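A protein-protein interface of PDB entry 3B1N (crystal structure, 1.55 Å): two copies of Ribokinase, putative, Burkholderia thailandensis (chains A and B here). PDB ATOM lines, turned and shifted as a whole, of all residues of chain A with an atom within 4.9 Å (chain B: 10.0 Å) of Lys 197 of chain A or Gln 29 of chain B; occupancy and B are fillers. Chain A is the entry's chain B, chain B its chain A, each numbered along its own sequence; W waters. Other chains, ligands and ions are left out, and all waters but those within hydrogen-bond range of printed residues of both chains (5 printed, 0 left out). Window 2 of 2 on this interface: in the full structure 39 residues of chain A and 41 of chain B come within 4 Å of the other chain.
N of Leu 32 of chain B touches NH2 of Arg 22 of chain A (3.7 Å). Tyr 194 of chain A touches Leu 26 of chain B (CE2 to CD1, 3.7 Å). CD2 of Tyr 194 of chain A touches O of His 31 of chain B, at 3.4 Å. Leu 32 of chain B touches Tyr 194 of chain A (O to CE2, 3.5 Å). Ile 33 of chain B touches Tyr 194 of chain A (CA to CE2, 3.7 Å). Asn 34 of chain B touches Glu 195 of chain A. Lys 197 of chain A touches Leu 26 of chain B. Gln 29 of chain B touches Lys 197 of chain A (NE2 to CB, 3.7 Å). Leu 198 of chain A touches Leu 26 of chain B (CD1 to CD1, 3.7 Å).
Along chain A the printed residues that touch a printed residue of chain B span positions 22 to 198. Printed residues of chain B that touch a printed residue of chain A: His 24, Leu 26, Pro 27, Gln 29, Val 30, His 31, Leu 32, Ile 33 and Asn 34. Hydrophobic or aromatic side chains of chain B within 4 Å of the printed part of chain A: His 24, Leu 26, Val 30, His 31 and Leu 32.
The backbone carbonyl oxygen (O) of Leu 32 of chain B lies within hydrogen-bond range of the backbone NH (N) of Leu 26 of chain B (2.8 Å).
Gln 29 of chain B touches just these residues of chain A: Arg 22 (2.7 Å), Asp 193 (3.0 Å) and Lys 197 (3.7 Å). Leu 198 of chain A touches one residue of chain B. Of the printed residues of chain A, Leu 26 of chain B touches Tyr 194, Lys 197 and Leu 198. Of the printed residues of chain A, Pro 27 of chain B touches Arg 22 (3.0 Å). Of the printed residues of chain A, His 24 of chain B touches Tyr 194 (2.6 Å). Of the printed residues of chain A, Leu 32 of chain B touches Arg 22 and Tyr 194. Printed residues of chain B within 4 Å of Glu 195 of chain A: Asn 34 (3.9 Å). Val 199 of chain A touches none of the printed residues of chain B. The nearest residue of chain A that does not touch Gln 29 of chain B is Tyr 194 of chain A (4.3 Å). The nearest printed residue of chain B that does not touch Tyr 194 of chain A is Gln 29 of chain B (4.3 Å).
No position is printed for both chains.
The backbone carbonyl oxygen (O) of Asn 34 of chain B sits close to the side-chain hydroxyl (OH) of Tyr 194 of chain A. NH2 of Arg 22 of chain A lies within hydrogen-bond range of O of Gln 29 of chain B, 2.7 Å away. The side-chain amide oxygen (OE1) of Gln 29 of chain B sits close to the side-chain carboxylate (OD2) of Asp 193 of chain A (3.0 Å). The backbone carbonyl oxygen (O) of Pro 27 of chain B is in hydrogen-bond range of the guanidinium group (NH1) of Arg 22 of chain A (3.0 Å). The backbone carbonyl oxygen (O) of His 24 of chain B lies within hydrogen-bond range of the side-chain hydroxyl (OH) of Tyr 194 of chain A (2.6 Å). ND1 of His 31 of chain B lies within hydrogen-bond range of OD1 of Asp 193 of chain A (2.8 Å). The backbone NH (N) of Val 30 of chain B is in hydrogen-bond range of the side-chain carboxylate (OD2) of Asp 193 of chain A, 2.8 Å away. The backbone carbonyl oxygen (O) of Val 30 of chain B is in hydrogen-bond range of the guanidinium group (NH2) of Arg 22 of chain A (3.5 Å).
Water W4 lies within hydrogen-bond range of the side-chain carboxylate of Glu 195 of chain A and the side-chain amide nitrogen of Asn 34 of chain B. Water W5 bridges the side-chain hydroxyl (OH) of Tyr 194 of chain A and a ring nitrogen (ND1) of His 24 of chain B. Water W1 bridges the backbone carbonyl oxygen (O) of Asp 193 of chain A (2.8 Å) and the side-chain amide oxygen (OE1) of Gln 29 of chain B (2.9 Å). Water W3 bridges NE of Arg 22 of chain A and O of Val 30 of chain B. Water W2 lies within hydrogen-bond range of O of Asn 34 of chain B (2.9 Å), OH of Tyr 194 of chain A (3.0 Å) and ND1 of His 24 of chain B (3.4 Å).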
ATOM      1  N   ARG A  22     -16.199  37.089 -12.835  1.00  0.00           N
ATOM      2  CA  ARG A  22     -17.412  37.859 -12.774  1.00  0.00           C
ATOM      3  C   ARG A  22     -17.200  39.286 -12.256  1.00  0.00           C
ATOM      4  O   ARG A  22     -18.020  40.143 -12.541  1.00  0.00           O
ATOM      5  CB  ARG A  22     -18.431  37.173 -11.848  1.00  0.00           C
ATOM      6  CG  ARG A  22     -19.039  35.933 -12.517  1.00  0.00           C
ATOM      7  CD  ARG A  22     -19.947  35.189 -11.486  1.00  0.00           C
ATOM      8  NE  ARG A  22     -20.499  33.937 -12.061  1.00  0.00           N
ATOM      9  CZ  ARG A  22     -21.685  33.828 -12.627  1.00  0.00           C
ATOM     10  NH1 ARG A  22     -22.466  34.891 -12.750  1.00  0.00           N
ATOM     11  NH2 ARG A  22     -22.075  32.621 -13.068  1.00  0.00           N
ATOM     12  N   ASP A 193     -22.670  22.099 -14.457  1.00  0.00           N
ATOM     13  CA  ASP A 193     -23.919  22.731 -14.849  1.00  0.00           C
ATOM     14  C   ASP A 193     -23.850  23.573 -16.128  1.00  0.00           C
ATOM     15  O   ASP A 193     -24.818  23.676 -16.869  1.00  0.00           O
ATOM     16  CB  ASP A 193     -24.567  23.488 -13.703  1.00  0.00           C
ATOM     17  CG  ASP A 193     -23.881  24.749 -13.379  1.00  0.00           C
ATOM     18  OD1 ASP A 193     -22.651  24.759 -13.150  1.00  0.00           O
ATOM     19  OD2 ASP A 193     -24.627  25.742 -13.301  1.00  0.00           O
ATOM     20  N   TYR A 194     -22.688  24.164 -16.364  1.00  0.00           N
ATOM     21  CA  TYR A 194     -22.463  24.939 -17.576  1.00  0.00           C
ATOM     22  C   TYR A 194     -22.587  23.992 -18.769  1.00  0.00           C
ATOM     23  O   TYR A 194     -23.287  24.274 -19.762  1.00  0.00           O
ATOM     24  CB  TYR A 194     -21.088  25.628 -17.520  1.00  0.00           C
ATOM     25  CG  TYR A 194     -20.697  26.393 -18.775  1.00  0.00           C
ATOM     26  CD1 TYR A 194     -20.120  25.738 -19.838  1.00  0.00           C
ATOM     27  CD2 TYR A 194     -20.934  27.759 -18.864  1.00  0.00           C
ATOM     28  CE1 TYR A 194     -19.753  26.434 -21.017  1.00  0.00           C
ATOM     29  CE2 TYR A 194     -20.570  28.450 -20.010  1.00  0.00           C
ATOM     30  CZ  TYR A 194     -19.990  27.798 -21.053  1.00  0.00           C
ATOM     31  OH  TYR A 194     -19.668  28.513 -22.193  1.00  0.00           O
ATOM     32  N   GLU A 195     -21.889  22.858 -18.694  1.00  0.00           N
ATOM     33  CA  GLU A 195     -21.953  21.884 -19.763  1.00  0.00           C
ATOM     34  C   GLU A 195     -23.366  21.326 -19.923  1.00  0.00           C
ATOM     35  O   GLU A 195     -23.805  21.052 -21.050  1.00  0.00           O
ATOM     36  CB  GLU A 195     -20.951  20.753 -19.449  1.00  0.00           C
ATOM     37  CG  GLU A 195     -19.478  21.212 -19.365  1.00  0.00           C
ATOM     38  CD  GLU A 195     -18.538  20.190 -18.618  1.00  0.00           C
ATOM     39  OE1 GLU A 195     -18.952  19.181 -17.900  1.00  0.00           O
ATOM     40  OE2 GLU A 195     -17.309  20.395 -18.808  1.00  0.00           O
ATOM     41  N   ALA A 196     -24.057  21.110 -18.793  1.00  0.00           N
ATOM     42  CA  ALA A 196     -25.418  20.558 -18.846  1.00  0.00           C
ATOM     43  C   ALA A 196     -26.301  21.509 -19.686  1.00  0.00           C
ATOM     44  O   ALA A 196     -27.068  21.052 -20.546  1.00  0.00           O
ATOM     45  CB  ALA A 196     -25.991  20.445 -17.458  1.00  0.00           C
ATOM     46  N   LYS A 197     -26.155  22.818 -19.464  1.00  0.00           N
ATOM     47  CA  LYS A 197     -26.904  23.802 -20.267  1.00  0.00           C
ATOM     48  C   LYS A 197     -26.590  23.678 -21.769  1.00  0.00           C
ATOM     49  O   LYS A 197     -27.500  23.674 -22.620  1.00  0.00           O
ATOM     50  CB  LYS A 197     -26.697  25.227 -19.747  1.00  0.00           C
ATOM     51  CG  LYS A 197     -27.419  26.305 -20.579  1.00  0.00           C
ATOM     52  CD  LYS A 197     -28.949  26.101 -20.466  1.00  0.00           C
ATOM     53  CE  LYS A 197     -29.711  27.178 -21.278  1.00  0.00           C
ATOM     54  NZ  LYS A 197     -31.042  27.330 -20.655  1.00  0.00           N
ATOM     55  N   LEU A 198     -25.310  23.535 -22.094  1.00  0.00           N
ATOM     56  CA  LEU A 198     -24.903  23.388 -23.479  1.00  0.00           C
ATOM     57  C   LEU A 198     -25.429  22.087 -24.067  1.00  0.00           C
ATOM     58  O   LEU A 198     -25.784  22.050 -25.256  1.00  0.00           O
ATOM     59  CB  LEU A 198     -23.372  23.464 -23.584  1.00  0.00           C
ATOM     60  CG  LEU A 198     -22.688  24.798 -23.872  1.00  0.00           C
ATOM     61  CD1 LEU A 198     -23.224  25.922 -23.030  1.00  0.00           C
ATOM     62  CD2 LEU A 198     -21.220  24.623 -23.676  1.00  0.00           C
ATOM     63  N   VAL A 199     -25.498  21.019 -23.259  1.00  0.00           N
ATOM     64  CA  VAL A 199     -26.037  19.744 -23.783  1.00  0.00           C
ATOM     65  C   VAL A 199     -27.533  19.879 -24.136  1.00  0.00           C
ATOM     66  O   VAL A 199     -27.972  19.410 -25.216  1.00  0.00           O
ATOM     67  CB  VAL A 199     -25.828  18.598 -22.776  1.00  0.00           C
ATOM     68  CG1 VAL A 199     -26.613  17.323 -23.237  1.00  0.00           C
ATOM     69  CG2 VAL A 199     -24.305  18.255 -22.669  1.00  0.00           C
ATOM     70  N   CYS A 200     -28.288  20.485 -23.222  1.00  0.00           N
ATOM     71  CA  CYS A 200     -29.731  20.735 -23.454  1.00  0.00           C
ATOM     72  C   CYS A 200     -29.890  21.583 -24.711  1.00  0.00           C
ATOM     73  O   CYS A 200     -30.684  21.250 -25.603  1.00  0.00           O
ATOM     74  CB  CYS A 200     -30.294  21.475 -22.277  1.00  0.00           C
ATOM     75  SG  CYS A 200     -30.508  20.461 -20.829  1.00  0.00           S
ATOM     76  N   ASP A 201     -29.114  22.661 -24.814  1.00  0.00           N
ATOM     77  CA  ASP A 201     -29.190  23.536 -26.010  1.00  0.00           C
ATOM     78  C   ASP A 201     -28.904  22.795 -27.309  1.00  0.00           C
ATOM     79  O   ASP A 201     -29.628  22.965 -28.302  1.00  0.00           O
ATOM     80  CB  ASP A 201     -28.234  24.715 -25.893  1.00  0.00           C
ATOM     81  CG  ASP A 201     -28.678  25.743 -24.875  1.00  0.00           C
ATOM     82  OD1 ASP A 201     -29.768  25.618 -24.245  1.00  0.00           O
ATOM     83  OD2 ASP A 201     -27.884  26.696 -24.689  1.00  0.00           O
ATOM     84  N   HIS B  24     -20.032  33.052 -24.979  1.00  0.00           N
ATOM     85  CA  HIS B  24     -19.845  31.803 -24.228  1.00  0.00           C
ATOM     86  C   HIS B  24     -20.034  32.004 -22.733  1.00  0.00           C
ATOM     87  O   HIS B  24     -19.851  31.059 -21.969  1.00  0.00           O
ATOM     88  CB  HIS B  24     -18.501  31.174 -24.573  1.00  0.00           C
ATOM     89  CG  HIS B  24     -18.407  30.813 -26.025  1.00  0.00           C
ATOM     90  ND1 HIS B  24     -18.911  29.632 -26.543  1.00  0.00           N
ATOM     91  CD2 HIS B  24     -17.992  31.541 -27.088  1.00  0.00           C
ATOM     92  CE1 HIS B  24     -18.740  29.626 -27.858  1.00  0.00           C
ATOM     93  NE2 HIS B  24     -18.169  30.768 -28.210  1.00  0.00           N
ATOM     94  N   ILE B  25     -20.384  33.219 -22.302  1.00  0.00           N
ATOM     95  CA  ILE B  25     -20.605  33.427 -20.881  1.00  0.00           C
ATOM     96  C   ILE B  25     -22.086  33.175 -20.570  1.00  0.00           C
ATOM     97  O   ILE B  25     -22.990  33.539 -21.336  1.00  0.00           O
ATOM     98  CB  ILE B  25     -20.090  34.809 -20.328  1.00  0.00           C
ATOM     99  CG1 ILE B  25     -20.749  35.978 -21.045  1.00  0.00           C
ATOM    100  CG2 ILE B  25     -18.556  34.899 -20.359  1.00  0.00           C
ATOM    101  CD1 ILE B  25     -20.616  37.263 -20.240  1.00  0.00           C
ATOM    102  N   LEU B  26     -22.313  32.468 -19.472  1.00  0.00           N
ATOM    103  CA  LEU B  26     -23.668  32.119 -19.045  1.00  0.00           C
ATOM    104  C   LEU B  26     -23.804  32.519 -17.586  1.00  0.00           C
ATOM    105  O   LEU B  26     -23.555  31.697 -16.668  1.00  0.00           O
ATOM    106  CB  LEU B  26     -23.913  30.604 -19.237  1.00  0.00           C
ATOM    107  CG  LEU B  26     -23.965  30.076 -20.670  1.00  0.00           C
ATOM    108  CD1 LEU B  26     -24.177  28.568 -20.583  1.00  0.00           C
ATOM    109  CD2 LEU B  26     -25.053  30.756 -21.521  1.00  0.00           C
ATOM    110  N   PRO B  27     -24.154  33.800 -17.338  1.00  0.00           N
ATOM    111  CA  PRO B  27     -24.167  34.324 -15.962  1.00  0.00           C
ATOM    112  C   PRO B  27     -25.167  33.620 -15.049  1.00  0.00           C
ATOM    113  O   PRO B  27     -24.936  33.584 -13.849  1.00  0.00           O
ATOM    114  CB  PRO B  27     -24.560  35.811 -16.134  1.00  0.00           C
ATOM    115  CG  PRO B  27     -25.101  35.923 -17.543  1.00  0.00           C
ATOM    116  CD  PRO B  27     -24.352  34.874 -18.336  1.00  0.00           C
ATOM    117  N   ASP B  28     -26.197  32.975 -15.613  1.00  0.00           N
ATOM    118  CA  ASP B  28     -27.176  32.261 -14.783  1.00  0.00           C
ATOM    119  C   ASP B  28     -26.722  30.901 -14.278  1.00  0.00           C
ATOM    120  O   ASP B  28     -27.361  30.325 -13.385  1.00  0.00           O
ATOM    121  CB  ASP B  28     -28.493  32.014 -15.550  1.00  0.00           C
ATOM    122  CG  ASP B  28     -29.222  33.288 -15.936  1.00  0.00           C
ATOM    123  OD1 ASP B  28     -28.977  34.369 -15.355  1.00  0.00           O
ATOM    124  OD2 ASP B  28     -30.100  33.174 -16.824  1.00  0.00           O
ATOM    125  N   GLN B  29     -25.656  30.343 -14.850  1.00  0.00           N
ATOM    126  CA  GLN B  29     -25.128  29.078 -14.335  1.00  0.00           C
ATOM    127  C   GLN B  29     -24.166  29.322 -13.160  1.00  0.00           C
ATOM    128  O   GLN B  29     -23.763  30.465 -12.927  1.00  0.00           O
ATOM    129  CB  GLN B  29     -24.417  28.316 -15.440  1.00  0.00           C
ATOM    130  CG  GLN B  29     -25.259  28.093 -16.695  1.00  0.00           C
ATOM    131  CD  GLN B  29     -26.522  27.319 -16.403  1.00  0.00           C
ATOM    132  OE1 GLN B  29     -26.560  26.438 -15.517  1.00  0.00           O
ATOM    133  NE2 GLN B  29     -27.561  27.652 -17.120  1.00  0.00           N
ATOM    134  N   VAL B  30     -23.787  28.280 -12.423  1.00  0.00           N
ATOM    135  CA  VAL B  30     -22.775  28.424 -11.370  1.00  0.00           C
ATOM    136  C   VAL B  30     -21.447  28.777 -12.011  1.00  0.00           C
ATOM    137  O   VAL B  30     -20.787  29.733 -11.611  1.00  0.00           O
ATOM    138  CB  VAL B  30     -22.664  27.122 -10.533  1.00  0.00           C
ATOM    139  CG1 VAL B  30     -21.407  27.090  -9.630  1.00  0.00           C
ATOM    140  CG2 VAL B  30     -23.951  26.942  -9.752  1.00  0.00           C
ATOM    141  N   HIS B  31     -21.059  27.994 -13.002  1.00  0.00           N
ATOM    142  CA  HIS B  31     -19.908  28.309 -13.787  1.00  0.00           C
ATOM    143  C   HIS B  31     -20.313  29.321 -14.898  1.00  0.00           C
ATOM    144  O   HIS B  31     -21.171  29.025 -15.726  1.00  0.00           O
ATOM    145  CB  HIS B  31     -19.327  27.014 -14.372  1.00  0.00           C
ATOM    146  CG  HIS B  31     -18.969  25.980 -13.338  1.00  0.00           C
ATOM    147  ND1 HIS B  31     -19.894  25.086 -12.820  1.00  0.00           N
ATOM    148  CD2 HIS B  31     -17.780  25.645 -12.769  1.00  0.00           C
ATOM    149  CE1 HIS B  31     -19.293  24.253 -11.981  1.00  0.00           C
ATOM    150  NE2 HIS B  31     -18.003  24.561 -11.949  1.00  0.00           N
ATOM    151  N   LEU B  32     -19.670  30.491 -14.883  1.00  0.00           N
ATOM    152  CA  LEU B  32     -19.818  31.560 -15.879  1.00  0.00           C
ATOM    153  C   LEU B  32     -19.349  31.112 -17.267  1.00  0.00           C
ATOM    154  O   LEU B  32     -20.015  31.405 -18.296  1.00  0.00           O
ATOM    155  CB  LEU B  32     -19.001  32.810 -15.455  1.00  0.00           C
ATOM    156  CG  LEU B  32     -19.105  34.006 -16.445  1.00  0.00           C
ATOM    157  CD1 LEU B  32     -20.499  34.585 -16.404  1.00  0.00           C
ATOM    158  CD2 LEU B  32     -18.053  35.077 -16.195  1.00  0.00           C
ATOM    159  N   ILE B  33     -18.214  30.419 -17.287  1.00  0.00           N
ATOM    160  CA  ILE B  33     -17.604  30.083 -18.563  1.00  0.00           C
ATOM    161  C   ILE B  33     -16.678  28.895 -18.419  1.00  0.00           C
ATOM    162  O   ILE B  33     -15.883  28.789 -17.473  1.00  0.00           O
ATOM    163  CB  ILE B  33     -16.917  31.305 -19.243  1.00  0.00           C
ATOM    164  CG1 ILE B  33     -16.404  30.890 -20.633  1.00  0.00           C
ATOM    165  CG2 ILE B  33     -15.778  31.830 -18.394  1.00  0.00           C
ATOM    166  CD1 ILE B  33     -15.980  32.017 -21.560  1.00  0.00           C
ATOM    167  N   ASN B  34     -16.911  27.930 -19.313  1.00  0.00           N
ATOM    168  CA  ASN B  34     -15.955  26.888 -19.588  1.00  0.00           C
ATOM    169  C   ASN B  34     -15.761  26.920 -21.081  1.00  0.00           C
ATOM    170  O   ASN B  34     -16.735  26.893 -21.866  1.00  0.00           O
ATOM    171  CB  ASN B  34     -16.495  25.508 -19.278  1.00  0.00           C
ATOM    172  CG  ASN B  34     -16.601  25.218 -17.826  1.00  0.00           C
ATOM    173  OD1 ASN B  34     -16.140  25.954 -16.932  1.00  0.00           O
ATOM    174  ND2 ASN B  34     -17.220  24.102 -17.560  1.00  0.00           N
HETATM  175  O   HOH W   1     -27.557  23.819 -16.289  1.00  0.00           O
HETATM  176  O   HOH W   2     -18.205  27.091 -24.393  1.00  0.00           O
HETATM  177  O   HOH W   3     -18.760  31.760 -11.732  1.00  0.00           O
HETATM  178  O   HOH W   4     -16.924  22.410 -20.377  1.00  0.00           O
HETATM  179  O   HOH W   5     -20.451  27.966 -24.828  1.00  0.00           O
